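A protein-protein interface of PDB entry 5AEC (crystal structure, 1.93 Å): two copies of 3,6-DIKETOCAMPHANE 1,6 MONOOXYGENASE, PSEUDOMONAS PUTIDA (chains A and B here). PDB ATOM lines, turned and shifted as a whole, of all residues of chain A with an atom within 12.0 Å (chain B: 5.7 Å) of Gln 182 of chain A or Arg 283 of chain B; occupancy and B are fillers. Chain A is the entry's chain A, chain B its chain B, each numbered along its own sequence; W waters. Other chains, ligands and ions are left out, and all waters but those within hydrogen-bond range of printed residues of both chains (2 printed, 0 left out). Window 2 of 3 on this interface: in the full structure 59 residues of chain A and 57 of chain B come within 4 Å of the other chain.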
ATOM      1  N   ARG A 156      14.691  31.687   4.114  1.00  0.00           N
ATOM      2  CA  ARG A 156      14.175  30.364   4.373  1.00  0.00           C
ATOM      3  C   ARG A 156      15.319  29.384   4.682  1.00  0.00           C
ATOM      4  O   ARG A 156      15.287  28.221   4.317  1.00  0.00           O
ATOM      5  CB  ARG A 156      13.252  29.889   3.226  1.00  0.00           C
ATOM      6  CG  ARG A 156      12.023  30.774   3.095  1.00  0.00           C
ATOM      7  CD  ARG A 156      11.034  30.345   2.036  1.00  0.00           C
ATOM      8  NE  ARG A 156      10.268  29.161   2.404  1.00  0.00           N
ATOM      9  CZ  ARG A 156      10.408  27.959   1.857  1.00  0.00           C
ATOM     10  NH1 ARG A 156      11.325  27.737   0.925  1.00  0.00           N
ATOM     11  NH2 ARG A 156       9.639  26.950   2.268  1.00  0.00           N
ATOM     12  N   GLU A 173      12.969  21.370   8.017  1.00  0.00           N
ATOM     13  CA  GLU A 173      11.873  20.504   7.572  1.00  0.00           C
ATOM     14  C   GLU A 173      11.689  19.342   8.593  1.00  0.00           C
ATOM     15  O   GLU A 173      12.673  18.843   9.153  1.00  0.00           O
ATOM     16  CB  GLU A 173      12.207  19.937   6.187  1.00  0.00           C
ATOM     17  CG  GLU A 173      12.359  20.960   5.048  1.00  0.00           C
ATOM     18  CD  GLU A 173      11.032  21.515   4.569  1.00  0.00           C
ATOM     19  OE1 GLU A 173      10.042  20.796   4.758  1.00  0.00           O
ATOM     20  OE2 GLU A 173      10.947  22.640   3.989  1.00  0.00           O
ATOM     21  N   LEU A 174      10.450  18.904   8.826  1.00  0.00           N
ATOM     22  CA  LEU A 174      10.198  17.719   9.662  1.00  0.00           C
ATOM     23  C   LEU A 174      10.759  16.442   8.998  1.00  0.00           C
ATOM     24  O   LEU A 174      10.859  16.370   7.765  1.00  0.00           O
ATOM     25  CB  LEU A 174       8.710  17.573  10.004  1.00  0.00           C
ATOM     26  CG  LEU A 174       8.127  18.575  11.023  1.00  0.00           C
ATOM     27  CD1 LEU A 174       6.610  18.465  11.101  1.00  0.00           C
ATOM     28  CD2 LEU A 174       8.753  18.411  12.404  1.00  0.00           C
ATOM     29  N   GLU A 175      11.095  15.452   9.828  1.00  0.00           N
ATOM     30  CA  GLU A 175      11.958  14.302   9.435  1.00  0.00           C
ATOM     31  C   GLU A 175      11.438  13.557   8.206  1.00  0.00           C
ATOM     32  O   GLU A 175      10.331  13.030   8.244  1.00  0.00           O
ATOM     33  CB  GLU A 175      12.074  13.310  10.598  1.00  0.00           C
ATOM     34  CG  GLU A 175      13.182  12.280  10.435  1.00  0.00           C
ATOM     35  CD  GLU A 175      13.461  11.517  11.723  1.00  0.00           C
ATOM     36  OE1 GLU A 175      12.501  10.991  12.325  1.00  0.00           O
ATOM     37  OE2 GLU A 175      14.636  11.452  12.141  1.00  0.00           O
ATOM     38  N   GLU A 181       5.402  16.783  -1.770  1.00  0.00           N
ATOM     39  CA  GLU A 181       5.711  18.196  -1.642  1.00  0.00           C
ATOM     40  C   GLU A 181       4.793  18.836  -0.584  1.00  0.00           C
ATOM     41  O   GLU A 181       5.195  19.778   0.101  1.00  0.00           O
ATOM     42  CB  GLU A 181       5.632  18.901  -3.008  1.00  0.00           C
ATOM     43  CG  GLU A 181       4.242  19.062  -3.633  1.00  0.00           C
ATOM     44  CD  GLU A 181       3.810  17.931  -4.559  1.00  0.00           C
ATOM     45  OE1 GLU A 181       4.520  16.913  -4.685  1.00  0.00           O
ATOM     46  OE2 GLU A 181       2.735  18.068  -5.181  1.00  0.00           O
ATOM     47  N   GLN A 182       3.581  18.295  -0.449  1.00  0.00           N
ATOM     48  CA  GLN A 182       2.547  18.775   0.492  1.00  0.00           C
ATOM     49  C   GLN A 182       2.881  18.846   1.994  1.00  0.00           C
ATOM     50  O   GLN A 182       2.132  19.467   2.755  1.00  0.00           O
ATOM     51  CB  GLN A 182       1.298  17.908   0.349  1.00  0.00           C
ATOM     52  CG  GLN A 182       1.503  16.450   0.763  1.00  0.00           C
ATOM     53  CD  GLN A 182       0.220  15.662   0.774  1.00  0.00           C
ATOM     54  OE1 GLN A 182      -0.020  14.831   1.657  1.00  0.00           O
ATOM     55  NE2 GLN A 182      -0.622  15.927  -0.205  1.00  0.00           N
ATOM     56  N   HIS A 183       3.944  18.166   2.427  1.00  0.00           N
ATOM     57  CA  HIS A 183       4.390  18.185   3.835  1.00  0.00           C
ATOM     58  C   HIS A 183       5.644  19.036   4.102  1.00  0.00           C
ATOM     59  O   HIS A 183       6.056  19.195   5.251  1.00  0.00           O
ATOM     60  CB  HIS A 183       4.569  16.746   4.334  1.00  0.00           C
ATOM     61  CG  HIS A 183       3.277  16.013   4.512  1.00  0.00           C
ATOM     62  ND1 HIS A 183       2.093  16.645   4.837  1.00  0.00           N
ATOM     63  CD2 HIS A 183       2.988  14.694   4.419  1.00  0.00           C
ATOM     64  CE1 HIS A 183       1.129  15.746   4.922  1.00  0.00           C
ATOM     65  NE2 HIS A 183       1.647  14.555   4.678  1.00  0.00           N
ATOM     66  N   LYS A 184       6.222  19.607   3.050  1.00  0.00           N
ATOM     67  CA  LYS A 184       7.291  20.587   3.190  1.00  0.00           C
ATOM     68  C   LYS A 184       6.744  21.864   3.835  1.00  0.00           C
ATOM     69  O   LYS A 184       5.537  22.037   3.997  1.00  0.00           O
ATOM     70  CB  LYS A 184       7.897  20.915   1.814  1.00  0.00           C
ATOM     71  CG  LYS A 184       8.450  19.684   1.095  1.00  0.00           C
ATOM     72  CD  LYS A 184       9.690  19.961   0.259  1.00  0.00           C
ATOM     73  CE  LYS A 184       9.478  21.107  -0.719  1.00  0.00           C
ATOM     74  NZ  LYS A 184      10.530  21.118  -1.769  1.00  0.00           N
ATOM     75  N   LEU A 185       7.629  22.784   4.162  1.00  0.00           N
ATOM     76  CA  LEU A 185       7.195  24.083   4.689  1.00  0.00           C
ATOM     77  C   LEU A 185       6.558  24.952   3.585  1.00  0.00           C
ATOM     78  O   LEU A 185       7.027  24.938   2.448  1.00  0.00           O
ATOM     79  CB  LEU A 185       8.387  24.779   5.321  1.00  0.00           C
ATOM     80  CG  LEU A 185       8.806  24.153   6.662  1.00  0.00           C
ATOM     81  CD1 LEU A 185      10.259  24.481   7.015  1.00  0.00           C
ATOM     82  CD2 LEU A 185       7.871  24.610   7.790  1.00  0.00           C
ATOM     83  N   ALA A 186       5.537  25.746   3.952  1.00  0.00           N
ATOM     84  CA  ALA A 186       4.993  26.796   3.091  1.00  0.00           C
ATOM     85  C   ALA A 186       6.099  27.751   2.682  1.00  0.00           C
ATOM     86  O   ALA A 186       7.086  27.919   3.405  1.00  0.00           O
ATOM     87  CB  ALA A 186       3.892  27.571   3.794  1.00  0.00           C
ATOM     88  N   ASP A 187       5.943  28.351   1.510  1.00  0.00           N
ATOM     89  CA  ASP A 187       6.880  29.353   1.037  1.00  0.00           C
ATOM     90  C   ASP A 187       6.182  30.702   0.997  1.00  0.00           C
ATOM     91  O   ASP A 187       5.501  31.039   0.013  1.00  0.00           O
ATOM     92  CB  ASP A 187       7.429  28.966  -0.329  1.00  0.00           C
ATOM     93  CG  ASP A 187       8.535  29.907  -0.818  1.00  0.00           C
ATOM     94  OD1 ASP A 187       8.787  30.999  -0.235  1.00  0.00           O
ATOM     95  OD2 ASP A 187       9.168  29.545  -1.826  1.00  0.00           O
ATOM     96  N   PHE A 188       6.390  31.481   2.067  1.00  0.00           N
ATOM     97  CA  PHE A 188       5.939  32.855   2.138  1.00  0.00           C
ATOM     98  C   PHE A 188       7.123  33.837   2.007  1.00  0.00           C
ATOM     99  O   PHE A 188       7.036  34.956   2.487  1.00  0.00           O
ATOM    100  CB  PHE A 188       5.143  33.089   3.409  1.00  0.00           C
ATOM    101  CG  PHE A 188       3.880  32.295   3.459  1.00  0.00           C
ATOM    102  CD1 PHE A 188       2.863  32.527   2.528  1.00  0.00           C
ATOM    103  CD2 PHE A 188       3.687  31.351   4.428  1.00  0.00           C
ATOM    104  CE1 PHE A 188       1.693  31.786   2.562  1.00  0.00           C
ATOM    105  CE2 PHE A 188       2.534  30.609   4.475  1.00  0.00           C
ATOM    106  CZ  PHE A 188       1.539  30.810   3.526  1.00  0.00           C
ATOM    107  N   PRO B  15      -1.661  22.109  -3.783  1.00  0.00           N
ATOM    108  CA  PRO B  15      -0.275  22.543  -3.851  1.00  0.00           C
ATOM    109  C   PRO B  15       0.059  23.035  -5.255  1.00  0.00           C
ATOM    110  O   PRO B  15      -0.338  22.407  -6.234  1.00  0.00           O
ATOM    111  CB  PRO B  15       0.499  21.288  -3.483  1.00  0.00           C
ATOM    112  CG  PRO B  15      -0.416  20.543  -2.588  1.00  0.00           C
ATOM    113  CD  PRO B  15      -1.806  20.823  -3.079  1.00  0.00           C
ATOM    114  N   ILE B  50       1.060  23.926   3.530  1.00  0.00           N
ATOM    115  CA  ILE B  50       0.914  24.070   2.062  1.00  0.00           C
ATOM    116  C   ILE B  50      -0.543  24.213   1.638  1.00  0.00           C
ATOM    117  O   ILE B  50      -0.883  25.113   0.858  1.00  0.00           O
ATOM    118  CB  ILE B  50       1.530  22.864   1.288  1.00  0.00           C
ATOM    119  CG1 ILE B  50       3.024  22.685   1.645  1.00  0.00           C
ATOM    120  CG2 ILE B  50       1.345  23.008  -0.234  1.00  0.00           C
ATOM    121  CD1 ILE B  50       3.953  23.729   1.074  1.00  0.00           C
ATOM    122  N   TRP B  51      -1.381  23.275   2.080  1.00  0.00           N
ATOM    123  CA  TRP B  51      -2.788  23.263   1.701  1.00  0.00           C
ATOM    124  C   TRP B  51      -3.564  24.364   2.416  1.00  0.00           C
ATOM    125  O   TRP B  51      -4.487  24.939   1.839  1.00  0.00           O
ATOM    126  CB  TRP B  51      -3.463  21.922   2.016  1.00  0.00           C
ATOM    127  CG  TRP B  51      -3.122  20.748   1.085  1.00  0.00           C
ATOM    128  CD1 TRP B  51      -2.012  19.958   1.134  1.00  0.00           C
ATOM    129  CD2 TRP B  51      -3.934  20.227   0.017  1.00  0.00           C
ATOM    130  NE1 TRP B  51      -2.067  18.986   0.157  1.00  0.00           N
ATOM    131  CE2 TRP B  51      -3.239  19.125  -0.539  1.00  0.00           C
ATOM    132  CE3 TRP B  51      -5.167  20.594  -0.535  1.00  0.00           C
ATOM    133  CZ2 TRP B  51      -3.751  18.380  -1.621  1.00  0.00           C
ATOM    134  CZ3 TRP B  51      -5.664  19.862  -1.615  1.00  0.00           C
ATOM    135  CH2 TRP B  51      -4.950  18.773  -2.153  1.00  0.00           C
ATOM    136  N   GLY B 278     -12.874  14.792  -2.881  1.00  0.00           N
ATOM    137  CA  GLY B 278     -12.261  13.476  -2.877  1.00  0.00           C
ATOM    138  C   GLY B 278     -10.769  13.524  -3.087  1.00  0.00           C
ATOM    139  O   GLY B 278     -10.028  12.818  -2.419  1.00  0.00           O
ATOM    140  N   TYR B 279     -10.334  14.377  -4.002  1.00  0.00           N
ATOM    141  CA  TYR B 279      -8.904  14.581  -4.247  1.00  0.00           C
ATOM    142  C   TYR B 279      -8.123  15.018  -2.995  1.00  0.00           C
ATOM    143  O   TYR B 279      -7.089  14.432  -2.654  1.00  0.00           O
ATOM    144  CB  TYR B 279      -8.714  15.599  -5.369  1.00  0.00           C
ATOM    145  CG  TYR B 279      -7.258  15.808  -5.731  1.00  0.00           C
ATOM    146  CD1 TYR B 279      -6.586  14.863  -6.501  1.00  0.00           C
ATOM    147  CD2 TYR B 279      -6.543  16.931  -5.273  1.00  0.00           C
ATOM    148  CE1 TYR B 279      -5.249  15.025  -6.827  1.00  0.00           C
ATOM    149  CE2 TYR B 279      -5.196  17.099  -5.583  1.00  0.00           C
ATOM    150  CZ  TYR B 279      -4.554  16.136  -6.370  1.00  0.00           C
ATOM    151  OH  TYR B 279      -3.235  16.243  -6.690  1.00  0.00           O
ATOM    152  N   CYS B 280      -8.638  16.032  -2.299  1.00  0.00           N
ATOM    153  CA  CYS B 280      -7.986  16.520  -1.083  1.00  0.00           C
ATOM    154  C   CYS B 280      -7.929  15.440  -0.004  1.00  0.00           C
ATOM    155  O   CYS B 280      -6.921  15.266   0.679  1.00  0.00           O
ATOM    156  CB  CYS B 280      -8.707  17.777  -0.536  1.00  0.00           C
ATOM    157  SG  CYS B 280      -7.928  18.382   0.969  1.00  0.00           S
ATOM    158  N   PHE B 281      -9.036  14.727   0.160  1.00  0.00           N
ATOM    159  CA  PHE B 281      -9.100  13.679   1.154  1.00  0.00           C
ATOM    160  C   PHE B 281      -8.127  12.535   0.856  1.00  0.00           C
ATOM    161  O   PHE B 281      -7.387  12.101   1.755  1.00  0.00           O
ATOM    162  CB  PHE B 281     -10.550  13.211   1.361  1.00  0.00           C
ATOM    163  CG  PHE B 281     -11.275  14.004   2.416  1.00  0.00           C
ATOM    164  CD1 PHE B 281     -11.116  13.673   3.748  1.00  0.00           C
ATOM    165  CD2 PHE B 281     -12.061  15.095   2.086  1.00  0.00           C
ATOM    166  CE1 PHE B 281     -11.741  14.406   4.734  1.00  0.00           C
ATOM    167  CE2 PHE B 281     -12.703  15.824   3.066  1.00  0.00           C
ATOM    168  CZ  PHE B 281     -12.543  15.480   4.393  1.00  0.00           C
ATOM    169  N   GLU B 282      -8.087  12.078  -0.393  1.00  0.00           N
ATOM    170  CA  GLU B 282      -7.197  10.951  -0.714  1.00  0.00           C
ATOM    171  C   GLU B 282      -5.728  11.347  -0.703  1.00  0.00           C
ATOM    172  O   GLU B 282      -4.906  10.619  -0.142  1.00  0.00           O
ATOM    173  CB  GLU B 282      -7.609  10.258  -2.025  1.00  0.00           C
ATOM    174  CG  GLU B 282      -8.767   9.296  -1.767  1.00  0.00           C
ATOM    175  CD  GLU B 282      -9.354   8.641  -2.998  1.00  0.00           C
ATOM    176  OE1 GLU B 282      -9.204   9.187  -4.109  1.00  0.00           O
ATOM    177  OE2 GLU B 282      -9.991   7.578  -2.834  1.00  0.00           O
ATOM    178  N   ARG B 283      -5.405  12.516  -1.253  1.00  0.00           N
ATOM    179  CA  ARG B 283      -4.015  12.980  -1.316  1.00  0.00           C
ATOM    180  C   ARG B 283      -3.461  13.437   0.035  1.00  0.00           C
ATOM    181  O   ARG B 283      -2.295  13.172   0.358  1.00  0.00           O
ATOM    182  CB  ARG B 283      -3.875  14.135  -2.330  1.00  0.00           C
ATOM    183  CG  ARG B 283      -4.251  13.747  -3.777  1.00  0.00           C
ATOM    184  CD  ARG B 283      -3.128  13.053  -4.568  1.00  0.00           C
ATOM    185  NE  ARG B 283      -3.040  11.608  -4.303  1.00  0.00           N
ATOM    186  CZ  ARG B 283      -3.931  10.659  -4.638  1.00  0.00           C
ATOM    187  NH1 ARG B 283      -5.067  10.930  -5.295  1.00  0.00           N
ATOM    188  NH2 ARG B 283      -3.672   9.395  -4.300  1.00  0.00           N
ATOM    189  N   TYR B 284      -4.297  14.101   0.837  1.00  0.00           N
ATOM    190  CA  TYR B 284      -3.822  14.837   1.993  1.00  0.00           C
ATOM    191  C   TYR B 284      -4.506  14.480   3.323  1.00  0.00           C
ATOM    192  O   TYR B 284      -3.836  14.103   4.282  1.00  0.00           O
ATOM    193  CB  TYR B 284      -3.982  16.322   1.672  1.00  0.00           C
ATOM    194  CG  TYR B 284      -3.553  17.251   2.778  1.00  0.00           C
ATOM    195  CD1 TYR B 284      -2.248  17.212   3.279  1.00  0.00           C
ATOM    196  CD2 TYR B 284      -4.435  18.200   3.289  1.00  0.00           C
ATOM    197  CE1 TYR B 284      -1.843  18.081   4.298  1.00  0.00           C
ATOM    198  CE2 TYR B 284      -4.050  19.065   4.309  1.00  0.00           C
ATOM    199  CZ  TYR B 284      -2.765  19.007   4.814  1.00  0.00           C
ATOM    200  OH  TYR B 284      -2.390  19.865   5.818  1.00  0.00           O
ATOM    201  N   LEU B 285      -5.820  14.640   3.412  1.00  0.00           N
ATOM    202  CA  LEU B 285      -6.484  14.571   4.720  1.00  0.00           C
ATOM    203  C   LEU B 285      -6.585  13.167   5.316  1.00  0.00           C
ATOM    204  O   LEU B 285      -6.286  12.993   6.499  1.00  0.00           O
ATOM    205  CB  LEU B 285      -7.861  15.239   4.689  1.00  0.00           C
ATOM    206  CG  LEU B 285      -7.852  16.761   4.538  1.00  0.00           C
ATOM    207  CD1 LEU B 285      -9.283  17.275   4.461  1.00  0.00           C
ATOM    208  CD2 LEU B 285      -7.093  17.434   5.693  1.00  0.00           C
ATOM    209  N   PRO B 287      -4.683  10.431   5.016  1.00  0.00           N
ATOM    210  CA  PRO B 287      -3.438  10.003   5.668  1.00  0.00           C
ATOM    211  C   PRO B 287      -3.108  10.697   6.986  1.00  0.00           C
ATOM    212  O   PRO B 287      -2.670  10.021   7.929  1.00  0.00           O
ATOM    213  CB  PRO B 287      -2.361  10.313   4.622  1.00  0.00           C
ATOM    214  CG  PRO B 287      -3.078  10.273   3.322  1.00  0.00           C
ATOM    215  CD  PRO B 287      -4.477  10.747   3.592  1.00  0.00           C
HETATM  216  O   HOH W   1       2.491  21.786   4.577  1.00  0.00           O
HETATM  217  O   HOH W   2      -1.005  13.707   4.337  1.00  0.00           O
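The guanidinium group (NH2) of Arg 156 of chain A is in hydrogen-bond range of the backbone carbonyl oxygen (O) of Leu 185 of chain A (3.3 Å).
O of Ala 186 of chain A is in hydrogen-bond range of NH2 of Arg 156 of chain A (3.0 Å).
The backbone NH (N) of Leu 185 of chain A is in hydrogen-bond range of the side-chain carboxylate (OE1) of Glu 173 of chain A (3.2 Å).
The side-chain amide oxygen (OE1) of Gln 182 of chain A lies within hydrogen-bond range of a ring nitrogen (NE2) of His 183 of chain A.
Among the printed residues, pairs that only touch across the chains: Lys 184 of chain A with Ile 50 of chain B, Gln 182 of chain A with Ile 50 of chain B, Leu 185 of chain A with Ile 50 of chain B, Gln 182 of chain A with Tyr 284 of chain B, Ala 186 of chain A with Ile 50 of chain B, His 183 of chain A with Tyr 284 of chain B and Glu 181 of chain A with Ile 50 of chain B.
Glu 175 of chain A touches none of the printed residues of chain B.
Printed residues of chain B within 4 Å of Gln 182 of chain A: Ile 50, Trp 51, Arg 283 and Tyr 284.
Of the printed residues of chain B, His 183 of chain A touches Tyr 284 (3.8 Å).
Printed residues of chain B within 4 Å of Lys 184 of chain A: Ile 50 (3.5 Å).
Printed residues of chain B within 4 Å of Leu 185 of chain A: Ile 50 (3.6 Å).
Asp 187 of chain A touches none of the printed residues of chain B.
No residue of chain A comes within 4 Å of Glu 282 of chain B.
Of the printed residues of chain A, Arg 283 of chain B touches Gln 182.
Tyr 284 of chain B touches just these residues of chain A: Gln 182 and His 183.
The nearest printed residue of chain A that does not touch Trp 51 of chain B is His 183 of chain A (6.4 Å).
Of the 12 printed residues of chain A, 6 touch a printed residue of chain B.
Hydrophobic or aromatic side chains of chain B that line the printed part of chain A: Ile 50, Trp 51 and Tyr 284.
Among the printed residues, 9 pairs touch across the chains.
Among the printed residues, no Asp or Glu carboxylate lies within 4 Å of a Lys or Arg side-chain nitrogen of the other chain.
Water W1 lies within hydrogen-bond range of N of Ile 50 of chain B (2.8 Å), O of Gln 182 of chain A (3.0 Å) and O of Lys 184 of chain A (3.1 Å).
Water W2 lies within hydrogen-bond range of NE2 of His 183 of chain A (2.8 Å), O of Tyr 284 of chain B (2.9 Å) and OE1 of Gln 182 of chain A (3.1 Å).
No position is printed for both chains.
Of the 9 pairs that touch across the chains among the printed residues, none has its exchanged pair printed and touching as well.
NE2 of Gln 182 of chain A lies close to NE1 of Trp 51 of chain B, 3.4 Å away.
The backbone carbonyl oxygen of Arg 283 of chain B sits close to the side-chain amide oxygen of Gln 182 of chain A, 3.1 Å away.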
